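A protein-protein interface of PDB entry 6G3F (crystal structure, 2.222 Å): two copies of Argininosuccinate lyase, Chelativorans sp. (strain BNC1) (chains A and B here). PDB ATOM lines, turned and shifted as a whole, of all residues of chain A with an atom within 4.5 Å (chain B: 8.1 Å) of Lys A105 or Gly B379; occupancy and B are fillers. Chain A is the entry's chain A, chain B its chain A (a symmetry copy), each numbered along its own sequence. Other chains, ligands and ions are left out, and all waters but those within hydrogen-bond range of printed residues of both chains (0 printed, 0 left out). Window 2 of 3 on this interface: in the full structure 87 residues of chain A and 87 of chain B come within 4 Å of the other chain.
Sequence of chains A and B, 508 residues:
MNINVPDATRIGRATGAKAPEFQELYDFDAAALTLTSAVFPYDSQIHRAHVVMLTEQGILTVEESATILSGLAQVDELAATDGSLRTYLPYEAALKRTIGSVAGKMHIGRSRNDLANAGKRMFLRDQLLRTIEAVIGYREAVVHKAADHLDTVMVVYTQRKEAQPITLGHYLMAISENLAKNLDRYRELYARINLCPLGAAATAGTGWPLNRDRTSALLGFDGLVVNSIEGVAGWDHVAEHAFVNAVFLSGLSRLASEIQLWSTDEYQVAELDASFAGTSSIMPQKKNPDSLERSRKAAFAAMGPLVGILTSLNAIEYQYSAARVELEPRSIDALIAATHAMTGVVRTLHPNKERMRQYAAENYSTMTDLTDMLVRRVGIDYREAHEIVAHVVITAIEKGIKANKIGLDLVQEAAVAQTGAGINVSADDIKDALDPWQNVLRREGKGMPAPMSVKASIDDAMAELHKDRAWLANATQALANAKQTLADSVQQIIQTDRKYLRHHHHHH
Among the printed residues, merely in contact across the chains: Gly A104 with Asp B381, Gly A104 with Tyr B382, Lys A105 with Ile B380, Lys A105 with Asp B381, His A107 with Arg B383 and Ile A108 with Val B375.
Of the printed residues of chain B, Lys A105 touches Gly B379, Ile B380 and Asp B381. Of chain A, only Lys A105 comes within 4 Å of Gly B379. Gly A104 touches two residues of chain B. Printed residues of chain A within 4 Å of Asp B381: Gly A104 and Lys A105. Of the printed residues of chain B, His A107 touches Arg B383. Of the printed residues of chain A, Ile B380 touches Lys A105. Ala B385 touches none of the printed residues of chain A. The nearest residue of chain B that does not touch Lys A105 is Tyr B382 (4.4 Å).
No position is printed for both chains.
O of Gly B379 is in hydrogen-bond range of NZ of Lys A105.
Hydrophobic or aromatic side chains of chain B within 4 Å of the printed part of chain A: Val B375 and Tyr B382. Of the 10 printed residues of chain A, 4 touch a printed residue of chain B. Printed residues of chain A that touch a printed residue of chain B: Gly A104, Lys A105, His A107 and Ile A108. Hydrophobic or aromatic side chains of chain A within 4 Å of the printed part of chain B: His A107 and Ile A108. Among the printed residues, 7 pairs touch across the chains. Among the printed residues, no Asp or Glu carboxylate lies within 4 Å of a Lys or Arg side-chain nitrogen of the other chain.
NZ of Lys A105 lies within salt-bridge range of OE2 of Glu A64. The side-chain carboxylate (OD2) of Asp B381 is in hydrogen-bond range of the backbone NH (N) of Glu B384 (3.0 Å). The side-chain carboxylate (OD2) of Asp B381 is in hydrogen-bond range of the backbone NH (N) of Arg B383, 3.1 Å away.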
ATOM      1  N   LEU A  54      -2.587 -15.626  -5.979  1.00  0.00           N
ATOM      2  CA  LEU A  54      -3.043 -15.140  -7.278  1.00  0.00           C
ATOM      3  C   LEU A  54      -4.335 -14.348  -7.134  1.00  0.00           C
ATOM      4  O   LEU A  54      -4.523 -13.321  -7.798  1.00  0.00           O
ATOM      5  CB  LEU A  54      -3.247 -16.307  -8.244  1.00  0.00           C
ATOM      6  CG  LEU A  54      -2.019 -17.000  -8.838  1.00  0.00           C
ATOM      7  CD1 LEU A  54      -2.477 -18.051  -9.836  1.00  0.00           C
ATOM      8  CD2 LEU A  54      -1.071 -16.010  -9.505  1.00  0.00           C
ATOM      9  N   LEU A  60      -6.535 -13.940 -10.442  1.00  0.00           N
ATOM     10  CA  LEU A  60      -7.714 -14.786 -10.543  1.00  0.00           C
ATOM     11  C   LEU A  60      -8.907 -14.053  -9.950  1.00  0.00           C
ATOM     12  O   LEU A  60      -8.767 -13.326  -8.962  1.00  0.00           O
ATOM     13  CB  LEU A  60      -7.515 -16.111  -9.797  1.00  0.00           C
ATOM     14  CG  LEU A  60      -6.420 -17.062 -10.282  1.00  0.00           C
ATOM     15  CD1 LEU A  60      -6.293 -18.232  -9.315  1.00  0.00           C
ATOM     16  CD2 LEU A  60      -6.712 -17.563 -11.685  1.00  0.00           C
ATOM     17  N   GLU A  64     -13.203 -17.835 -10.098  1.00  0.00           N
ATOM     18  CA  GLU A  64     -12.169 -18.749 -10.570  1.00  0.00           C
ATOM     19  C   GLU A  64     -11.461 -19.423  -9.400  1.00  0.00           C
ATOM     20  O   GLU A  64     -11.317 -20.650  -9.368  1.00  0.00           O
ATOM     21  CB  GLU A  64     -11.166 -17.988 -11.437  1.00  0.00           C
ATOM     22  CG  GLU A  64     -11.714 -17.563 -12.789  1.00  0.00           C
ATOM     23  CD  GLU A  64     -10.770 -16.640 -13.537  1.00  0.00           C
ATOM     24  OE1 GLU A  64     -10.041 -15.871 -12.876  1.00  0.00           O
ATOM     25  OE2 GLU A  64     -10.754 -16.688 -14.787  1.00  0.00           O
ATOM     26  N   VAL A 102     -10.758 -23.679 -16.397  1.00  0.00           N
ATOM     27  CA  VAL A 102     -10.183 -22.751 -15.430  1.00  0.00           C
ATOM     28  C   VAL A 102      -9.061 -23.398 -14.631  1.00  0.00           C
ATOM     29  O   VAL A 102      -8.229 -22.694 -14.048  1.00  0.00           O
ATOM     30  CB  VAL A 102     -11.288 -22.216 -14.493  1.00  0.00           C
ATOM     31  CG1 VAL A 102     -11.799 -23.320 -13.565  1.00  0.00           C
ATOM     32  CG2 VAL A 102     -10.790 -21.015 -13.701  1.00  0.00           C
ATOM     33  N   ALA A 103      -9.018 -24.732 -14.588  1.00  0.00           N
ATOM     34  CA  ALA A 103      -7.969 -25.423 -13.848  1.00  0.00           C
ATOM     35  C   ALA A 103      -6.584 -24.979 -14.301  1.00  0.00           C
ATOM     36  O   ALA A 103      -5.661 -24.875 -13.486  1.00  0.00           O
ATOM     37  CB  ALA A 103      -8.126 -26.934 -14.020  1.00  0.00           C
ATOM     38  N   GLY A 104      -6.420 -24.711 -15.598  1.00  0.00           N
ATOM     39  CA  GLY A 104      -5.118 -24.345 -16.127  1.00  0.00           C
ATOM     40  C   GLY A 104      -4.565 -23.047 -15.573  1.00  0.00           C
ATOM     41  O   GLY A 104      -3.355 -22.809 -15.669  1.00  0.00           O
ATOM     42  N   LYS A 105      -5.415 -22.201 -14.994  1.00  0.00           N
ATOM     43  CA  LYS A 105      -4.958 -20.911 -14.495  1.00  0.00           C
ATOM     44  C   LYS A 105      -4.226 -21.003 -13.163  1.00  0.00           C
ATOM     45  O   LYS A 105      -3.575 -20.030 -12.767  1.00  0.00           O
ATOM     46  CB  LYS A 105      -6.138 -19.947 -14.356  1.00  0.00           C
ATOM     47  CG  LYS A 105      -6.704 -19.475 -15.683  1.00  0.00           C
ATOM     48  CD  LYS A 105      -7.573 -18.240 -15.502  1.00  0.00           C
ATOM     49  CE  LYS A 105      -8.051 -17.695 -16.838  1.00  0.00           C
ATOM     50  NZ  LYS A 105      -8.777 -16.407 -16.678  1.00  0.00           N
ATOM     51  N   MET A 106      -4.309 -22.133 -12.457  1.00  0.00           N
ATOM     52  CA  MET A 106      -3.556 -22.260 -11.215  1.00  0.00           C
ATOM     53  C   MET A 106      -2.052 -22.297 -11.450  1.00  0.00           C
ATOM     54  O   MET A 106      -1.289 -22.133 -10.491  1.00  0.00           O
ATOM     55  CB  MET A 106      -3.997 -23.512 -10.443  1.00  0.00           C
ATOM     56  CG  MET A 106      -3.463 -24.855 -10.951  1.00  0.00           C
ATOM     57  SD  MET A 106      -3.372 -26.066  -9.609  1.00  0.00           S
ATOM     58  CE  MET A 106      -3.165 -27.593 -10.514  1.00  0.00           C
ATOM     59  N   HIS A 107      -1.610 -22.500 -12.689  1.00  0.00           N
ATOM     60  CA  HIS A 107      -0.193 -22.559 -13.017  1.00  0.00           C
ATOM     61  C   HIS A 107       0.352 -21.217 -13.493  1.00  0.00           C
ATOM     62  O   HIS A 107       1.513 -21.146 -13.913  1.00  0.00           O
ATOM     63  CB  HIS A 107       0.052 -23.627 -14.083  1.00  0.00           C
ATOM     64  CG  HIS A 107       1.396 -24.278 -13.988  1.00  0.00           C
ATOM     65  ND1 HIS A 107       1.927 -24.715 -12.794  1.00  0.00           N
ATOM     66  CD2 HIS A 107       2.315 -24.573 -14.939  1.00  0.00           C
ATOM     67  CE1 HIS A 107       3.117 -25.248 -13.012  1.00  0.00           C
ATOM     68  NE2 HIS A 107       3.375 -25.174 -14.305  1.00  0.00           N
ATOM     69  N   ILE A 108      -0.457 -20.155 -13.443  1.00  0.00           N
ATOM     70  CA  ILE A 108       0.004 -18.841 -13.879  1.00  0.00           C
ATOM     71  C   ILE A 108       1.200 -18.420 -13.041  1.00  0.00           C
ATOM     72  O   ILE A 108       1.168 -18.484 -11.807  1.00  0.00           O
ATOM     73  CB  ILE A 108      -1.133 -17.812 -13.784  1.00  0.00           C
ATOM     74  CG1 ILE A 108      -2.169 -18.063 -14.882  1.00  0.00           C
ATOM     75  CG2 ILE A 108      -0.589 -16.381 -13.901  1.00  0.00           C
ATOM     76  CD1 ILE A 108      -3.443 -17.265 -14.714  1.00  0.00           C
ATOM     77  N   ASP B 372       1.987 -15.957 -21.761  1.00  0.00           N
ATOM     78  CA  ASP B 372       1.410 -15.129 -20.705  1.00  0.00           C
ATOM     79  C   ASP B 372       0.550 -14.013 -21.288  1.00  0.00           C
ATOM     80  O   ASP B 372      -0.483 -13.651 -20.714  1.00  0.00           O
ATOM     81  CB  ASP B 372       2.518 -14.534 -19.832  1.00  0.00           C
ATOM     82  CG  ASP B 372       3.171 -15.557 -18.913  1.00  0.00           C
ATOM     83  OD1 ASP B 372       2.519 -16.559 -18.557  1.00  0.00           O
ATOM     84  OD2 ASP B 372       4.340 -15.345 -18.530  1.00  0.00           O
ATOM     85  N   MET B 373       0.967 -13.450 -22.425  1.00  0.00           N
ATOM     86  CA  MET B 373       0.213 -12.355 -23.026  1.00  0.00           C
ATOM     87  C   MET B 373      -1.165 -12.821 -23.471  1.00  0.00           C
ATOM     88  O   MET B 373      -2.157 -12.108 -23.282  1.00  0.00           O
ATOM     89  CB  MET B 373       0.987 -11.769 -24.205  1.00  0.00           C
ATOM     90  CG  MET B 373       0.306 -10.573 -24.858  1.00  0.00           C
ATOM     91  SD  MET B 373      -0.818 -11.034 -26.189  1.00  0.00           S
ATOM     92  CE  MET B 373       0.344 -11.550 -27.448  1.00  0.00           C
ATOM     93  N   LEU B 374      -1.250 -14.013 -24.067  1.00  0.00           N
ATOM     94  CA  LEU B 374      -2.553 -14.552 -24.439  1.00  0.00           C
ATOM     95  C   LEU B 374      -3.446 -14.682 -23.212  1.00  0.00           C
ATOM     96  O   LEU B 374      -4.589 -14.213 -23.207  1.00  0.00           O
ATOM     97  CB  LEU B 374      -2.393 -15.903 -25.144  1.00  0.00           C
ATOM     98  CG  LEU B 374      -1.509 -15.950 -26.397  1.00  0.00           C
ATOM     99  CD1 LEU B 374      -1.713 -17.264 -27.134  1.00  0.00           C
ATOM    100  CD2 LEU B 374      -1.768 -14.775 -27.332  1.00  0.00           C
ATOM    101  N   VAL B 375      -2.928 -15.289 -22.144  1.00  0.00           N
ATOM    102  CA  VAL B 375      -3.717 -15.452 -20.926  1.00  0.00           C
ATOM    103  C   VAL B 375      -4.198 -14.097 -20.429  1.00  0.00           C
ATOM    104  O   VAL B 375      -5.374 -13.915 -20.088  1.00  0.00           O
ATOM    105  CB  VAL B 375      -2.892 -16.183 -19.852  1.00  0.00           C
ATOM    106  CG1 VAL B 375      -3.670 -16.282 -18.539  1.00  0.00           C
ATOM    107  CG2 VAL B 375      -2.493 -17.560 -20.352  1.00  0.00           C
ATOM    108  N   ARG B 376      -3.294 -13.122 -20.395  1.00  0.00           N
ATOM    109  CA  ARG B 376      -3.609 -11.811 -19.845  1.00  0.00           C
ATOM    110  C   ARG B 376      -4.616 -11.064 -20.714  1.00  0.00           C
ATOM    111  O   ARG B 376      -5.529 -10.413 -20.194  1.00  0.00           O
ATOM    112  CB  ARG B 376      -2.319 -11.011 -19.722  1.00  0.00           C
ATOM    113  CG  ARG B 376      -2.392  -9.741 -18.878  1.00  0.00           C
ATOM    114  CD  ARG B 376      -1.081  -8.962 -18.951  1.00  0.00           C
ATOM    115  NE  ARG B 376      -0.549  -8.916 -20.311  1.00  0.00           N
ATOM    116  CZ  ARG B 376       0.580  -8.310 -20.669  1.00  0.00           C
ATOM    117  NH1 ARG B 376       1.334  -7.679 -19.777  1.00  0.00           N
ATOM    118  NH2 ARG B 376       0.956  -8.342 -21.938  1.00  0.00           N
ATOM    119  N   ARG B 377      -4.464 -11.138 -22.039  1.00  0.00           N
ATOM    120  CA  ARG B 377      -5.245 -10.281 -22.927  1.00  0.00           C
ATOM    121  C   ARG B 377      -6.621 -10.859 -23.239  1.00  0.00           C
ATOM    122  O   ARG B 377      -7.608 -10.116 -23.269  1.00  0.00           O
ATOM    123  CB  ARG B 377      -4.477 -10.031 -24.230  1.00  0.00           C
ATOM    124  CG  ARG B 377      -3.385  -8.963 -24.146  1.00  0.00           C
ATOM    125  CD  ARG B 377      -3.911  -7.667 -23.548  1.00  0.00           C
ATOM    126  NE  ARG B 377      -3.274  -6.479 -24.117  1.00  0.00           N
ATOM    127  CZ  ARG B 377      -3.895  -5.539 -24.829  1.00  0.00           C
ATOM    128  NH1 ARG B 377      -5.197  -5.611 -25.077  1.00  0.00           N
ATOM    129  NH2 ARG B 377      -3.205  -4.505 -25.291  1.00  0.00           N
ATOM    130  N   VAL B 378      -6.717 -12.164 -23.488  1.00  0.00           N
ATOM    131  CA  VAL B 378      -7.989 -12.781 -23.852  1.00  0.00           C
ATOM    132  C   VAL B 378      -8.557 -13.666 -22.755  1.00  0.00           C
ATOM    133  O   VAL B 378      -9.724 -14.081 -22.860  1.00  0.00           O
ATOM    134  CB  VAL B 378      -7.877 -13.579 -25.169  1.00  0.00           C
ATOM    135  CG1 VAL B 378      -7.501 -12.658 -26.316  1.00  0.00           C
ATOM    136  CG2 VAL B 378      -6.863 -14.674 -25.051  1.00  0.00           C
ATOM    137  N   GLY B 379      -7.788 -13.973 -21.715  1.00  0.00           N
ATOM    138  CA  GLY B 379      -8.325 -14.651 -20.555  1.00  0.00           C
ATOM    139  C   GLY B 379      -8.393 -16.159 -20.639  1.00  0.00           C
ATOM    140  O   GLY B 379      -8.970 -16.781 -19.739  1.00  0.00           O
ATOM    141  N   ILE B 380      -7.834 -16.772 -21.685  1.00  0.00           N
ATOM    142  CA  ILE B 380      -7.784 -18.233 -21.729  1.00  0.00           C
ATOM    143  C   ILE B 380      -6.863 -18.751 -20.629  1.00  0.00           C
ATOM    144  O   ILE B 380      -5.988 -18.040 -20.118  1.00  0.00           O
ATOM    145  CB  ILE B 380      -7.334 -18.740 -23.111  1.00  0.00           C
ATOM    146  CG1 ILE B 380      -6.009 -18.091 -23.525  1.00  0.00           C
ATOM    147  CG2 ILE B 380      -8.423 -18.481 -24.145  1.00  0.00           C
ATOM    148  CD1 ILE B 380      -5.397 -18.686 -24.782  1.00  0.00           C
ATOM    149  N   ASP B 381      -7.072 -20.011 -20.251  1.00  0.00           N
ATOM    150  CA  ASP B 381      -6.224 -20.627 -19.244  1.00  0.00           C
ATOM    151  C   ASP B 381      -4.822 -20.844 -19.807  1.00  0.00           C
ATOM    152  O   ASP B 381      -4.597 -20.804 -21.021  1.00  0.00           O
ATOM    153  CB  ASP B 381      -6.817 -21.956 -18.774  1.00  0.00           C
ATOM    154  CG  ASP B 381      -6.832 -23.003 -19.863  1.00  0.00           C
ATOM    155  OD1 ASP B 381      -7.748 -22.965 -20.712  1.00  0.00           O
ATOM    156  OD2 ASP B 381      -5.928 -23.865 -19.868  1.00  0.00           O
ATOM    157  N   TYR B 382      -3.865 -21.074 -18.905  1.00  0.00           N
ATOM    158  CA  TYR B 382      -2.473 -21.146 -19.337  1.00  0.00           C
ATOM    159  C   TYR B 382      -2.217 -22.379 -20.194  1.00  0.00           C
ATOM    160  O   TYR B 382      -1.433 -22.323 -21.147  1.00  0.00           O
ATOM    161  CB  TYR B 382      -1.524 -21.138 -18.140  1.00  0.00           C
ATOM    162  CG  TYR B 382      -0.098 -20.950 -18.589  1.00  0.00           C
ATOM    163  CD1 TYR B 382       0.422 -19.680 -18.775  1.00  0.00           C
ATOM    164  CD2 TYR B 382       0.713 -22.040 -18.878  1.00  0.00           C
ATOM    165  CE1 TYR B 382       1.716 -19.495 -19.208  1.00  0.00           C
ATOM    166  CE2 TYR B 382       2.011 -21.866 -19.315  1.00  0.00           C
ATOM    167  CZ  TYR B 382       2.506 -20.589 -19.480  1.00  0.00           C
ATOM    168  OH  TYR B 382       3.797 -20.398 -19.916  1.00  0.00           O
ATOM    169  N   ARG B 383      -2.860 -23.504 -19.871  1.00  0.00           N
ATOM    170  CA  ARG B 383      -2.598 -24.730 -20.619  1.00  0.00           C
ATOM    171  C   ARG B 383      -3.027 -24.590 -22.074  1.00  0.00           C
ATOM    172  O   ARG B 383      -2.345 -25.084 -22.979  1.00  0.00           O
ATOM    173  CB  ARG B 383      -3.307 -25.916 -19.957  1.00  0.00           C
ATOM    174  CG  ARG B 383      -2.904 -27.284 -20.514  1.00  0.00           C
ATOM    175  CD  ARG B 383      -1.395 -27.498 -20.440  1.00  0.00           C
ATOM    176  NE  ARG B 383      -0.871 -27.204 -19.106  1.00  0.00           N
ATOM    177  CZ  ARG B 383       0.330 -26.687 -18.855  1.00  0.00           C
ATOM    178  NH1 ARG B 383       1.162 -26.381 -19.844  1.00  0.00           N
ATOM    179  NH2 ARG B 383       0.700 -26.463 -17.601  1.00  0.00           N
ATOM    180  N   GLU B 384      -4.151 -23.912 -22.322  1.00  0.00           N
ATOM    181  CA  GLU B 384      -4.602 -23.711 -23.697  1.00  0.00           C
ATOM    182  C   GLU B 384      -3.675 -22.754 -24.439  1.00  0.00           C
ATOM    183  O   GLU B 384      -3.253 -23.029 -25.568  1.00  0.00           O
ATOM    184  CB  GLU B 384      -6.037 -23.185 -23.712  1.00  0.00           C
ATOM    185  CG  GLU B 384      -6.797 -23.534 -24.984  1.00  0.00           C
ATOM    186  CD  GLU B 384      -8.042 -22.689 -25.179  1.00  0.00           C
ATOM    187  OE1 GLU B 384      -8.471 -22.021 -24.214  1.00  0.00           O
ATOM    188  OE2 GLU B 384      -8.589 -22.692 -26.302  1.00  0.00           O
ATOM    189  N   ALA B 385      -3.351 -21.617 -23.817  1.00  0.00           N
ATOM    190  CA  ALA B 385      -2.390 -20.696 -24.413  1.00  0.00           C
ATOM    191  C   ALA B 385      -1.074 -21.405 -24.711  1.00  0.00           C
ATOM    192  O   ALA B 385      -0.438 -21.153 -25.741  1.00  0.00           O
ATOM    193  CB  ALA B 385      -2.157 -19.510 -23.477  1.00  0.00           C
ATOM    194  N   ILE B 423      -7.746 -15.451 -32.368  1.00  0.00           N
ATOM    195  CA  ILE B 423      -7.476 -14.951 -31.025  1.00  0.00           C
ATOM    196  C   ILE B 423      -7.214 -13.451 -31.096  1.00  0.00           C
ATOM    197  O   ILE B 423      -6.526 -12.969 -32.004  1.00  0.00           O
ATOM    198  CB  ILE B 423      -6.294 -15.704 -30.375  1.00  0.00           C
ATOM    199  CG1 ILE B 423      -6.170 -15.308 -28.909  1.00  0.00           C
ATOM    200  CG2 ILE B 423      -4.992 -15.448 -31.132  1.00  0.00           C
ATOM    201  CD1 ILE B 423      -5.387 -16.298 -28.082  1.00  0.00           C
ATOM    202  N   ASN B 424      -7.727 -12.717 -30.105  1.00  0.00           N
ATOM    203  CA  ASN B 424      -7.830 -11.257 -30.168  1.00  0.00           C
ATOM    204  C   ASN B 424      -6.581 -10.659 -29.528  1.00  0.00           C
ATOM    205  O   ASN B 424      -6.550 -10.338 -28.339  1.00  0.00           O
ATOM    206  CB  ASN B 424      -9.099 -10.790 -29.456  1.00  0.00           C
ATOM    207  CG  ASN B 424      -9.297  -9.284 -29.513  1.00  0.00           C
ATOM    208  OD1 ASN B 424      -8.899  -8.631 -30.488  1.00  0.00           O
ATOM    209  ND2 ASN B 424      -9.910  -8.726 -28.466  1.00  0.00           N
ATOM    210  N   VAL B 425      -5.515 -10.553 -30.325  1.00  0.00           N
ATOM    211  CA  VAL B 425      -4.312  -9.835 -29.923  1.00  0.00           C
ATOM    212  C   VAL B 425      -3.768  -9.071 -31.125  1.00  0.00           C
ATOM    213  O   VAL B 425      -4.004  -9.429 -32.282  1.00  0.00           O
ATOM    214  CB  VAL B 425      -3.222 -10.773 -29.345  1.00  0.00           C
ATOM    215  CG1 VAL B 425      -3.750 -11.516 -28.125  1.00  0.00           C
ATOM    216  CG2 VAL B 425      -2.718 -11.754 -30.396  1.00  0.00           C
